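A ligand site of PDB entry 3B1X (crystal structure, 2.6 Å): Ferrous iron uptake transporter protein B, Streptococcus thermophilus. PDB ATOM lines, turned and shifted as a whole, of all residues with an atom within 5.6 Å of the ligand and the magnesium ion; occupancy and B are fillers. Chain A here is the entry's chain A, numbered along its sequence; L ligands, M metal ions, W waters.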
ATOM      1  N   GLY A  10     -32.300  21.578 -34.253  1.00  0.00           N
ATOM      2  CA  GLY A  10     -33.012  21.414 -32.996  1.00  0.00           C
ATOM      3  C   GLY A  10     -33.249  22.747 -32.332  1.00  0.00           C
ATOM      4  O   GLY A  10     -32.680  23.763 -32.749  1.00  0.00           O
ATOM      5  N   ASN A  11     -34.101  22.720 -31.302  1.00  0.00           N
ATOM      6  CA  ASN A  11     -34.436  23.891 -30.487  1.00  0.00           C
ATOM      7  C   ASN A  11     -33.218  24.649 -29.979  1.00  0.00           C
ATOM      8  O   ASN A  11     -32.160  24.045 -29.797  1.00  0.00           O
ATOM      9  CB  ASN A  11     -35.303  23.476 -29.289  1.00  0.00           C
ATOM     10  CG  ASN A  11     -36.722  23.051 -29.689  1.00  0.00           C
ATOM     11  OD1 ASN A  11     -37.072  22.965 -30.871  1.00  0.00           O
ATOM     12  ND2 ASN A  11     -37.532  22.774 -28.684  1.00  0.00           N
ATOM     13  N   PRO A  12     -33.342  25.982 -29.769  1.00  0.00           N
ATOM     14  CA  PRO A  12     -32.233  26.691 -29.121  1.00  0.00           C
ATOM     15  C   PRO A  12     -32.056  26.192 -27.679  1.00  0.00           C
ATOM     16  O   PRO A  12     -33.047  25.834 -27.053  1.00  0.00           O
ATOM     17  CB  PRO A  12     -32.689  28.154 -29.127  1.00  0.00           C
ATOM     18  CG  PRO A  12     -33.692  28.228 -30.224  1.00  0.00           C
ATOM     19  CD  PRO A  12     -34.405  26.919 -30.193  1.00  0.00           C
ATOM     20  N   ASN A  13     -30.805  26.174 -27.202  1.00  0.00           N
ATOM     21  CA  ASN A  13     -30.452  25.731 -25.832  1.00  0.00           C
ATOM     22  C   ASN A  13     -30.546  24.200 -25.649  1.00  0.00           C
ATOM     23  O   ASN A  13     -30.640  23.699 -24.526  1.00  0.00           O
ATOM     24  CB  ASN A  13     -31.263  26.519 -24.768  1.00  0.00           C
ATOM     25  CG  ASN A  13     -30.598  26.561 -23.390  1.00  0.00           C
ATOM     26  OD1 ASN A  13     -29.500  26.045 -23.168  1.00  0.00           O
ATOM     27  ND2 ASN A  13     -31.291  27.190 -22.442  1.00  0.00           N
ATOM     28  N   SER A  14     -30.528  23.466 -26.774  1.00  0.00           N
ATOM     29  CA  SER A  14     -30.594  22.004 -26.778  1.00  0.00           C
ATOM     30  C   SER A  14     -29.220  21.326 -26.721  1.00  0.00           C
ATOM     31  O   SER A  14     -29.121  20.174 -26.303  1.00  0.00           O
ATOM     32  CB  SER A  14     -31.371  21.486 -27.993  1.00  0.00           C
ATOM     33  OG  SER A  14     -30.746  21.876 -29.204  1.00  0.00           O
ATOM     34  N   GLY A  15     -28.179  22.035 -27.160  1.00  0.00           N
ATOM     35  CA  GLY A  15     -26.811  21.534 -27.062  1.00  0.00           C
ATOM     36  C   GLY A  15     -26.129  21.157 -28.350  1.00  0.00           C
ATOM     37  O   GLY A  15     -25.267  20.282 -28.347  1.00  0.00           O
ATOM     38  N   LYS A  16     -26.501  21.815 -29.448  1.00  0.00           N
ATOM     39  CA  LYS A  16     -25.963  21.530 -30.785  1.00  0.00           C
ATOM     40  C   LYS A  16     -24.478  21.880 -30.927  1.00  0.00           C
ATOM     41  O   LYS A  16     -23.702  21.061 -31.433  1.00  0.00           O
ATOM     42  CB  LYS A  16     -26.746  22.262 -31.882  1.00  0.00           C
ATOM     43  CG  LYS A  16     -28.204  21.868 -32.025  1.00  0.00           C
ATOM     44  CD  LYS A  16     -28.936  22.673 -33.098  1.00  0.00           C
ATOM     45  CE  LYS A  16     -29.088  24.143 -32.735  1.00  0.00           C
ATOM     46  NZ  LYS A  16     -29.812  24.358 -31.448  1.00  0.00           N
ATOM     47  N   THR A  17     -24.103  23.081 -30.485  1.00  0.00           N
ATOM     48  CA  THR A  17     -22.716  23.566 -30.556  1.00  0.00           C
ATOM     49  C   THR A  17     -21.805  22.761 -29.619  1.00  0.00           C
ATOM     50  O   THR A  17     -20.655  22.460 -29.972  1.00  0.00           O
ATOM     51  CB  THR A  17     -22.617  25.077 -30.261  1.00  0.00           C
ATOM     52  OG1 THR A  17     -23.614  25.787 -31.020  1.00  0.00           O
ATOM     53  CG2 THR A  17     -21.265  25.629 -30.633  1.00  0.00           C
ATOM     54  N   SER A  18     -22.320  22.429 -28.435  1.00  0.00           N
ATOM     55  CA  SER A  18     -21.617  21.613 -27.463  1.00  0.00           C
ATOM     56  C   SER A  18     -21.206  20.293 -28.108  1.00  0.00           C
ATOM     57  O   SER A  18     -20.065  19.845 -27.935  1.00  0.00           O
ATOM     58  CB  SER A  18     -22.479  21.364 -26.232  1.00  0.00           C
ATOM     59  OG  SER A  18     -22.917  22.596 -25.693  1.00  0.00           O
ATOM     60  N   LEU A  19     -22.144  19.706 -28.852  1.00  0.00           N
ATOM     61  CA  LEU A  19     -21.906  18.477 -29.619  1.00  0.00           C
ATOM     62  C   LEU A  19     -20.950  18.760 -30.782  1.00  0.00           C
ATOM     63  O   LEU A  19     -20.020  17.988 -31.013  1.00  0.00           O
ATOM     64  CB  LEU A  19     -23.214  17.838 -30.104  1.00  0.00           C
ATOM     65  CG  LEU A  19     -24.110  17.137 -29.076  1.00  0.00           C
ATOM     66  CD1 LEU A  19     -25.510  16.983 -29.610  1.00  0.00           C
ATOM     67  CD2 LEU A  19     -23.584  15.777 -28.651  1.00  0.00           C
ATOM     68  N   ARG A  29     -18.880  29.145 -29.704  1.00  0.00           N
ATOM     69  CA  ARG A  29     -19.595  29.734 -28.559  1.00  0.00           C
ATOM     70  C   ARG A  29     -20.768  28.863 -28.096  1.00  0.00           C
ATOM     71  O   ARG A  29     -21.660  28.512 -28.877  1.00  0.00           O
ATOM     72  CB  ARG A  29     -20.018  31.181 -28.838  1.00  0.00           C
ATOM     73  CG  ARG A  29     -18.850  32.157 -28.891  1.00  0.00           C
ATOM     74  CD  ARG A  29     -19.296  33.608 -28.819  1.00  0.00           C
ATOM     75  NE  ARG A  29     -18.144  34.512 -28.673  1.00  0.00           N
ATOM     76  CZ  ARG A  29     -18.202  35.833 -28.536  1.00  0.00           C
ATOM     77  NH1 ARG A  29     -19.365  36.468 -28.511  1.00  0.00           N
ATOM     78  NH2 ARG A  29     -17.078  36.535 -28.420  1.00  0.00           N
ATOM     79  N   VAL A  30     -20.712  28.541 -26.812  1.00  0.00           N
ATOM     80  CA  VAL A  30     -21.668  27.703 -26.093  1.00  0.00           C
ATOM     81  C   VAL A  30     -22.111  28.482 -24.859  1.00  0.00           C
ATOM     82  O   VAL A  30     -21.283  28.868 -24.035  1.00  0.00           O
ATOM     83  CB  VAL A  30     -21.021  26.353 -25.656  1.00  0.00           C
ATOM     84  CG1 VAL A  30     -21.881  25.600 -24.673  1.00  0.00           C
ATOM     85  CG2 VAL A  30     -20.730  25.476 -26.857  1.00  0.00           C
ATOM     86  N   GLY A  31     -23.418  28.713 -24.751  1.00  0.00           N
ATOM     87  CA  GLY A  31     -24.003  29.425 -23.615  1.00  0.00           C
ATOM     88  C   GLY A  31     -25.283  28.767 -23.131  1.00  0.00           C
ATOM     89  O   GLY A  31     -25.991  28.131 -23.909  1.00  0.00           O
ATOM     90  N   ASN A  32     -25.568  28.930 -21.833  1.00  0.00           N
ATOM     91  CA  ASN A  32     -26.734  28.300 -21.193  1.00  0.00           C
ATOM     92  C   ASN A  32     -28.044  29.107 -21.291  1.00  0.00           C
ATOM     93  O   ASN A  32     -28.838  29.159 -20.347  1.00  0.00           O
ATOM     94  CB  ASN A  32     -26.396  27.940 -19.736  1.00  0.00           C
ATOM     95  CG  ASN A  32     -26.081  29.162 -18.873  1.00  0.00           C
ATOM     96  OD1 ASN A  32     -25.613  30.184 -19.362  1.00  0.00           O
ATOM     97  ND2 ASN A  32     -26.347  29.042 -17.587  1.00  0.00           N
ATOM     98  N   TRP A  33     -28.251  29.723 -22.454  1.00  0.00           N
ATOM     99  CA  TRP A  33     -29.464  30.489 -22.754  1.00  0.00           C
ATOM    100  C   TRP A  33     -29.815  30.331 -24.252  1.00  0.00           C
ATOM    101  O   TRP A  33     -28.898  30.188 -25.071  1.00  0.00           O
ATOM    102  CB  TRP A  33     -29.296  31.963 -22.364  1.00  0.00           C
ATOM    103  CG  TRP A  33     -28.275  32.734 -23.157  1.00  0.00           C
ATOM    104  CD1 TRP A  33     -28.511  33.477 -24.281  1.00  0.00           C
ATOM    105  CD2 TRP A  33     -26.874  32.830 -22.900  1.00  0.00           C
ATOM    106  NE1 TRP A  33     -27.343  34.032 -24.742  1.00  0.00           N
ATOM    107  CE2 TRP A  33     -26.316  33.660 -23.909  1.00  0.00           C
ATOM    108  CE3 TRP A  33     -26.018  32.303 -21.915  1.00  0.00           C
ATOM    109  CZ2 TRP A  33     -24.948  33.971 -23.967  1.00  0.00           C
ATOM    110  CZ3 TRP A  33     -24.649  32.614 -21.973  1.00  0.00           C
ATOM    111  CH2 TRP A  33     -24.133  33.442 -22.990  1.00  0.00           C
ATOM    112  N   PRO A  34     -31.114  30.350 -24.609  1.00  0.00           N
ATOM    113  CA  PRO A  34     -31.497  30.246 -26.029  1.00  0.00           C
ATOM    114  C   PRO A  34     -30.973  31.397 -26.912  1.00  0.00           C
ATOM    115  O   PRO A  34     -31.036  32.559 -26.522  1.00  0.00           O
ATOM    116  CB  PRO A  34     -33.042  30.278 -25.997  1.00  0.00           C
ATOM    117  CG  PRO A  34     -33.405  30.788 -24.655  1.00  0.00           C
ATOM    118  CD  PRO A  34     -32.313  30.330 -23.738  1.00  0.00           C
ATOM    119  N   GLY A  35     -30.457  31.044 -28.095  1.00  0.00           N
ATOM    120  CA  GLY A  35     -30.005  32.018 -29.090  1.00  0.00           C
ATOM    121  C   GLY A  35     -28.540  32.445 -29.099  1.00  0.00           C
ATOM    122  O   GLY A  35     -28.242  33.620 -29.307  1.00  0.00           O
ATOM    123  N   VAL A  36     -27.639  31.483 -28.883  1.00  0.00           N
ATOM    124  CA  VAL A  36     -26.195  31.758 -28.877  1.00  0.00           C
ATOM    125  C   VAL A  36     -25.605  31.811 -30.301  1.00  0.00           C
ATOM    126  O   VAL A  36     -25.033  32.825 -30.696  1.00  0.00           O
ATOM    127  CB  VAL A  36     -25.425  30.770 -27.940  1.00  0.00           C
ATOM    128  CG1 VAL A  36     -23.909  30.877 -28.109  1.00  0.00           C
ATOM    129  CG2 VAL A  36     -25.803  31.035 -26.484  1.00  0.00           C
ATOM    130  N   THR A  37     -25.759  30.717 -31.059  1.00  0.00           N
ATOM    131  CA  THR A  37     -25.302  30.622 -32.454  1.00  0.00           C
ATOM    132  C   THR A  37     -26.180  31.495 -33.344  1.00  0.00           C
ATOM    133  O   THR A  37     -27.406  31.425 -33.275  1.00  0.00           O
ATOM    134  CB  THR A  37     -25.347  29.176 -32.989  1.00  0.00           C
ATOM    135  OG1 THR A  37     -24.698  28.291 -32.054  1.00  0.00           O
ATOM    136  CG2 THR A  37     -24.676  29.047 -34.338  1.00  0.00           C
ATOM    137  N   ASP A  55     -23.009  23.388 -37.874  1.00  0.00           N
ATOM    138  CA  ASP A  55     -23.691  23.964 -36.725  1.00  0.00           C
ATOM    139  C   ASP A  55     -24.536  25.105 -37.257  1.00  0.00           C
ATOM    140  O   ASP A  55     -24.092  25.873 -38.099  1.00  0.00           O
ATOM    141  CB  ASP A  55     -22.727  24.493 -35.650  1.00  0.00           C
ATOM    142  CG  ASP A  55     -23.446  24.853 -34.354  1.00  0.00           C
ATOM    143  OD1 ASP A  55     -24.545  24.306 -34.091  1.00  0.00           O
ATOM    144  OD2 ASP A  55     -22.925  25.677 -33.574  1.00  0.00           O
ATOM    145  N   LEU A  56     -25.763  25.197 -36.747  1.00  0.00           N
ATOM    146  CA  LEU A  56     -26.737  26.186 -37.205  1.00  0.00           C
ATOM    147  C   LEU A  56     -27.535  26.747 -36.024  1.00  0.00           C
ATOM    148  O   LEU A  56     -27.698  26.044 -35.026  1.00  0.00           O
ATOM    149  CB  LEU A  56     -27.676  25.550 -38.230  1.00  0.00           C
ATOM    150  CG  LEU A  56     -27.115  25.168 -39.608  1.00  0.00           C
ATOM    151  CD1 LEU A  56     -27.890  24.000 -40.194  1.00  0.00           C
ATOM    152  CD2 LEU A  56     -27.096  26.358 -40.558  1.00  0.00           C
ATOM    153  N   PRO A  57     -28.027  28.006 -36.123  1.00  0.00           N
ATOM    154  CA  PRO A  57     -28.843  28.553 -35.032  1.00  0.00           C
ATOM    155  C   PRO A  57     -30.069  27.684 -34.771  1.00  0.00           C
ATOM    156  O   PRO A  57     -30.592  27.065 -35.703  1.00  0.00           O
ATOM    157  CB  PRO A  57     -29.298  29.907 -35.575  1.00  0.00           C
ATOM    158  CG  PRO A  57     -28.271  30.285 -36.584  1.00  0.00           C
ATOM    159  CD  PRO A  57     -27.834  28.999 -37.210  1.00  0.00           C
ATOM    160  N   GLY A  58     -30.492  27.627 -33.513  1.00  0.00           N
ATOM    161  CA  GLY A  58     -31.645  26.839 -33.104  1.00  0.00           C
ATOM    162  C   GLY A  58     -32.952  27.347 -33.666  1.00  0.00           C
ATOM    163  O   GLY A  58     -33.076  28.532 -33.978  1.00  0.00           O
ATOM    164  N   ASN A 115     -30.197  14.330 -26.563  1.00  0.00           N
ATOM    165  CA  ASN A 115     -29.224  15.003 -25.725  1.00  0.00           C
ATOM    166  C   ASN A 115     -29.720  15.268 -24.317  1.00  0.00           C
ATOM    167  O   ASN A 115     -30.917  15.160 -24.044  1.00  0.00           O
ATOM    168  CB  ASN A 115     -28.743  16.296 -26.402  1.00  0.00           C
ATOM    169  CG  ASN A 115     -27.411  16.776 -25.859  1.00  0.00           C
ATOM    170  OD1 ASN A 115     -26.528  15.976 -25.543  1.00  0.00           O
ATOM    171  ND2 ASN A 115     -27.249  18.094 -25.773  1.00  0.00           N
ATOM    172  N   MET A 116     -28.775  15.612 -23.439  1.00  0.00           N
ATOM    173  CA  MET A 116     -28.991  15.974 -22.026  1.00  0.00           C
ATOM    174  C   MET A 116     -29.583  14.822 -21.194  1.00  0.00           C
ATOM    175  O   MET A 116     -30.336  15.049 -20.242  1.00  0.00           O
ATOM    176  CB  MET A 116     -29.809  17.259 -21.886  1.00  0.00           C
ATOM    177  CG  MET A 116     -29.070  18.481 -22.377  1.00  0.00           C
ATOM    178  SD  MET A 116     -30.013  19.984 -22.281  1.00  0.00           S
ATOM    179  CE  MET A 116     -28.892  21.097 -23.089  1.00  0.00           C
ATOM    180  N   ILE A 117     -29.214  13.607 -21.587  1.00  0.00           N
ATOM    181  CA  ILE A 117     -29.666  12.367 -20.931  1.00  0.00           C
ATOM    182  C   ILE A 117     -29.165  12.297 -19.462  1.00  0.00           C
ATOM    183  O   ILE A 117     -29.818  11.669 -18.620  1.00  0.00           O
ATOM    184  CB  ILE A 117     -29.286  11.094 -21.784  1.00  0.00           C
ATOM    185  CG1 ILE A 117     -30.217   9.913 -21.482  1.00  0.00           C
ATOM    186  CG2 ILE A 117     -27.794  10.750 -21.687  1.00  0.00           C
ATOM    187  CD1 ILE A 117     -31.536   9.967 -22.237  1.00  0.00           C
ATOM    188  N   ASP A 118     -28.026  12.951 -19.189  1.00  0.00           N
ATOM    189  CA  ASP A 118     -27.432  13.031 -17.844  1.00  0.00           C
ATOM    190  C   ASP A 118     -28.299  13.804 -16.847  1.00  0.00           C
ATOM    191  O   ASP A 118     -28.363  13.457 -15.677  1.00  0.00           O
ATOM    192  CB  ASP A 118     -26.026  13.645 -17.900  1.00  0.00           C
ATOM    193  CG  ASP A 118     -26.023  15.066 -18.444  1.00  0.00           C
ATOM    194  OD1 ASP A 118     -26.332  15.254 -19.646  1.00  0.00           O
ATOM    195  OD2 ASP A 118     -25.708  16.004 -17.677  1.00  0.00           O
ATOM    196  N   VAL A 119     -28.951  14.856 -17.353  1.00  0.00           N
ATOM    197  CA  VAL A 119     -29.883  15.686 -16.577  1.00  0.00           C
ATOM    198  C   VAL A 119     -31.120  14.862 -16.247  1.00  0.00           C
ATOM    199  O   VAL A 119     -31.604  14.901 -15.108  1.00  0.00           O
ATOM    200  CB  VAL A 119     -30.311  16.976 -17.343  1.00  0.00           C
ATOM    201  CG1 VAL A 119     -31.167  17.902 -16.467  1.00  0.00           C
ATOM    202  CG2 VAL A 119     -29.106  17.745 -17.865  1.00  0.00           C
ATOM    203  N   THR A 143     -27.557  10.791 -25.785  1.00  0.00           N
ATOM    204  CA  THR A 143     -26.267  11.499 -25.721  1.00  0.00           C
ATOM    205  C   THR A 143     -26.154  12.490 -24.570  1.00  0.00           C
ATOM    206  O   THR A 143     -27.149  12.962 -24.020  1.00  0.00           O
ATOM    207  CB  THR A 143     -25.949  12.281 -27.044  1.00  0.00           C
ATOM    208  OG1 THR A 143     -26.885  13.347 -27.223  1.00  0.00           O
ATOM    209  CG2 THR A 143     -25.962  11.374 -28.264  1.00  0.00           C
ATOM    210  N   SER A 144     -24.900  12.787 -24.211  1.00  0.00           N
ATOM    211  CA  SER A 144     -24.586  13.804 -23.227  1.00  0.00           C
ATOM    212  C   SER A 144     -23.324  14.500 -23.714  1.00  0.00           C
ATOM    213  O   SER A 144     -22.311  13.846 -23.939  1.00  0.00           O
ATOM    214  CB  SER A 144     -24.385  13.196 -21.831  1.00  0.00           C
ATOM    215  OG  SER A 144     -24.134  14.209 -20.876  1.00  0.00           O
ATOM    216  N   ALA A 145     -23.406  15.819 -23.895  1.00  0.00           N
ATOM    217  CA  ALA A 145     -22.255  16.616 -24.308  1.00  0.00           C
ATOM    218  C   ALA A 145     -21.394  16.943 -23.099  1.00  0.00           C
ATOM    219  O   ALA A 145     -20.192  17.222 -23.234  1.00  0.00           O
ATOM    220  CB  ALA A 145     -22.700  17.871 -25.007  1.00  0.00           C
ATOM    221  N   LEU A 146     -22.013  16.904 -21.915  1.00  0.00           N
ATOM    222  CA  LEU A 146     -21.358  17.166 -20.641  1.00  0.00           C
ATOM    223  C   LEU A 146     -20.559  15.956 -20.177  1.00  0.00           C
ATOM    224  O   LEU A 146     -19.387  16.088 -19.807  1.00  0.00           O
ATOM    225  CB  LEU A 146     -22.402  17.546 -19.573  1.00  0.00           C
ATOM    226  CG  LEU A 146     -21.954  18.361 -18.359  1.00  0.00           C
ATOM    227  CD1 LEU A 146     -21.903  19.850 -18.717  1.00  0.00           C
ATOM    228  CD2 LEU A 146     -22.867  18.140 -17.168  1.00  0.00           C
ATOM    229  N   LYS A 147     -21.200  14.788 -20.192  1.00  0.00           N
ATOM    230  CA  LYS A 147     -20.572  13.530 -19.789  1.00  0.00           C
ATOM    231  C   LYS A 147     -19.771  12.867 -20.921  1.00  0.00           C
ATOM    232  O   LYS A 147     -19.067  11.878 -20.687  1.00  0.00           O
ATOM    233  CB  LYS A 147     -21.646  12.560 -19.240  1.00  0.00           C
ATOM    234  CG  LYS A 147     -22.177  12.899 -17.848  1.00  0.00           C
ATOM    235  CD  LYS A 147     -21.197  12.496 -16.744  1.00  0.00           C
ATOM    236  CE  LYS A 147     -21.804  12.632 -15.358  1.00  0.00           C
ATOM    237  NZ  LYS A 147     -20.828  12.221 -14.304  1.00  0.00           N
HETATM  238  P1  LIG L   1     -28.238  27.588 -29.895  1.00  0.00           P
HETATM  239  O1  LIG L   1     -29.062  26.852 -30.877  1.00  0.00           O
HETATM  240  O2  LIG L   1     -28.917  28.994 -29.507  1.00  0.00           O
HETATM  241  O3  LIG L   1     -26.821  28.040 -30.489  1.00  0.00           O
HETATM  242  N1  LIG L   1     -27.926  26.797 -28.532  1.00  0.00           N
HETATM  243  P2  LIG L   1     -27.266  25.313 -28.762  1.00  0.00           P
HETATM  244  O4  LIG L   1     -28.235  24.357 -29.366  1.00  0.00           O
HETATM  245  O5  LIG L   1     -25.969  25.481 -29.703  1.00  0.00           O
HETATM  246  O6  LIG L   1     -26.838  24.790 -27.300  1.00  0.00           O
HETATM  247  P3  LIG L   1     -25.339  24.794 -26.671  1.00  0.00           P
HETATM  248  O7  LIG L   1     -24.398  23.963 -27.458  1.00  0.00           O
HETATM  249  O8  LIG L   1     -24.879  26.351 -26.645  1.00  0.00           O
HETATM  250  O9  LIG L   1     -25.577  24.295 -25.191  1.00  0.00           O
HETATM  251  C1  LIG L   1     -26.515  24.981 -24.329  1.00  0.00           C
HETATM  252  C2  LIG L   1     -26.204  24.747 -22.811  1.00  0.00           C
HETATM  253  O10 LIG L   1     -26.524  23.372 -22.484  1.00  0.00           O
HETATM  254  C3  LIG L   1     -24.731  24.962 -22.452  1.00  0.00           C
HETATM  255  O11 LIG L   1     -24.645  25.565 -21.153  1.00  0.00           O
HETATM  256  C4  LIG L   1     -24.167  23.541 -22.423  1.00  0.00           C
HETATM  257  O12 LIG L   1     -23.055  23.469 -21.535  1.00  0.00           O
HETATM  258  C5  LIG L   1     -25.366  22.741 -21.901  1.00  0.00           C
HETATM  259  N2  LIG L   1     -25.415  21.344 -22.389  1.00  0.00           N
HETATM  260  C6  LIG L   1     -25.284  20.923 -23.648  1.00  0.00           C
HETATM  261  N3  LIG L   1     -25.377  19.593 -23.690  1.00  0.00           N
HETATM  262  C7  LIG L   1     -25.562  19.159 -22.450  1.00  0.00           C
HETATM  263  C8  LIG L   1     -25.724  17.889 -21.901  1.00  0.00           C
HETATM  264  O13 LIG L   1     -25.713  16.880 -22.613  1.00  0.00           O
HETATM  265  N4  LIG L   1     -25.915  17.756 -20.518  1.00  0.00           N
HETATM  266  C9  LIG L   1     -25.923  18.915 -19.723  1.00  0.00           C
HETATM  267  N5  LIG L   1     -26.096  18.802 -18.412  1.00  0.00           N
HETATM  268  N6  LIG L   1     -25.764  20.136 -20.285  1.00  0.00           N
HETATM  269  C10 LIG L   1     -25.588  20.277 -21.607  1.00  0.00           C
HETATM  270 MG    MG M   1     -25.372  26.685 -31.047  1.00  0.00          MG
HETATM  271  O   HOH W   1     -29.290  30.257 -31.773  1.00  0.00           O
HETATM  272  O   HOH W   2     -24.470  27.695 -29.188  1.00  0.00           O
HETATM  273  O   HOH W   3     -26.201  25.935 -32.836  1.00  0.00           O
HETATM  274  O   HOH W   4     -27.352  27.872 -26.117  1.00  0.00           O
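Water W2 lies within hydrogen-bond range of O8 of the ligand and O of Arg 29. Water W3 lies within hydrogen-bond range of OD1 of Asp 55 (2.6 Å) and O of Leu 56 (2.7 Å). Water W1 lies within hydrogen-bond range of O2 of the ligand (2.6 Å), O of Thr 37 (2.7 Å) and N of Gly 58 (3.4 Å). Water W4 lies within hydrogen-bond range of O of Gly 31, N1 of the ligand and O of Trp 33.
N1 of the ligand sits close to N of Asn 13 (3.2 Å). Asn 11 touches the ligand. CA of Pro 12 touches O1 of the ligand, 3.6 Å away. OG of Ser 14 touches O4 of the ligand, 3.5 Å away. Val 30 touches the ligand. CB of Asn 32 touches O11 of the ligand, at 3.3 Å. Val 119 touches the ligand. CA of Ser 144 touches O13 of the ligand, at 3.3 Å. Leu 146 touches the ligand. Hydrophobic or aromatic side chains that line the ligand: Pro 12, Val 30, Val 36, Met 116, Val 119, Ala 145 and Leu 146. Of the 33 residues printed, 22 come within 4 Å of the ligand. The nearest printed residue that does not touch the ligand is Pro 34 (4.1 Å).
The magnesium ion is bound by O5 of the ligand (1.9 Å), OG1 of Thr 17 (2.0 Å), OG1 of Thr 37 (2.0 Å), O3 of the ligand (2.1 Å), water W3 (2.1 Å) and water W2 (2.3 Å). The magnesium ion has six donor atoms within binding distance.
The side-chain hydroxyl of Thr 17 lies close to the side-chain carboxylate of Asp 55 (2.6 Å). The side-chain amino group (NZ) of Lys 16 is in hydrogen-bond range of the side-chain hydroxyl (OG) of Ser 14 (3.5 Å). The backbone carbonyl oxygen of Asn 11 is in hydrogen-bond range of the side-chain amino group of Lys 16 (2.9 Å). NZ of Lys 16 is in hydrogen-bond range of O of Gly 10 (3.2 Å). ND2 of Asn 115 is in hydrogen-bond range of O of Ser 14. The side-chain hydroxyl (OG) of Ser 144 is in hydrogen-bond range of the backbone NH (N) of Lys 147, at 3.1 Å. N of Met 116 lies within hydrogen-bond range of O of Thr 143 (3.2 Å). The backbone carbonyl oxygen of Asn 11 lies within hydrogen-bond range of the side-chain hydroxyl of Ser 14 (2.7 Å).
The backbone NH (N) of Thr 17 sits at hydrogen-bond distance from an oxygen (O7) of the ligand. The backbone NH (N) of Thr 37 sits close to an oxygen (O3) of the ligand (2.9 Å). The backbone NH (N) of Lys 16 sits at hydrogen-bond distance from an oxygen (O4) of the ligand (3.1 Å). An oxygen (O4) of the ligand is in salt-bridge range of the side-chain amino group of Lys 16. The backbone NH of Ser 18 is in hydrogen-bond range of an oxygen (O7) of the ligand. OG of Ser 18 sits at hydrogen-bond distance from O7 of the ligand, 2.7 Å away. OD1 of Asp 118 lies within hydrogen-bond range of N4 of the ligand, at 2.7 Å. O13 of the ligand is in hydrogen-bond range of N of Ala 145, at 2.8 Å. O2 of the ligand sits at hydrogen-bond distance from N of Val 36 (2.9 Å). N of Gly 35 is in hydrogen-bond range of O2 of the ligand. An oxygen (O6) of the ligand is in hydrogen-bond range of the backbone NH (N) of Gly 15 (3.1 Å). An oxygen (O1) of the ligand is in hydrogen-bond range of the backbone NH of Gly 58, at 3.1 Å. The side-chain amide oxygen (OD1) of Asn 115 sits close to an oxygen (O13) of the ligand. N of Gly 31 lies within hydrogen-bond range of O8 of the ligand, 3.4 Å away. An oxygen (O13) of the ligand is in hydrogen-bond range of the backbone NH of Met 116 (3.4 Å).
Residues that only touch the magnesium ion: Asp 55. Along chain A the residues within 4 Å of the magnesium ion span positions 17 to 55.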
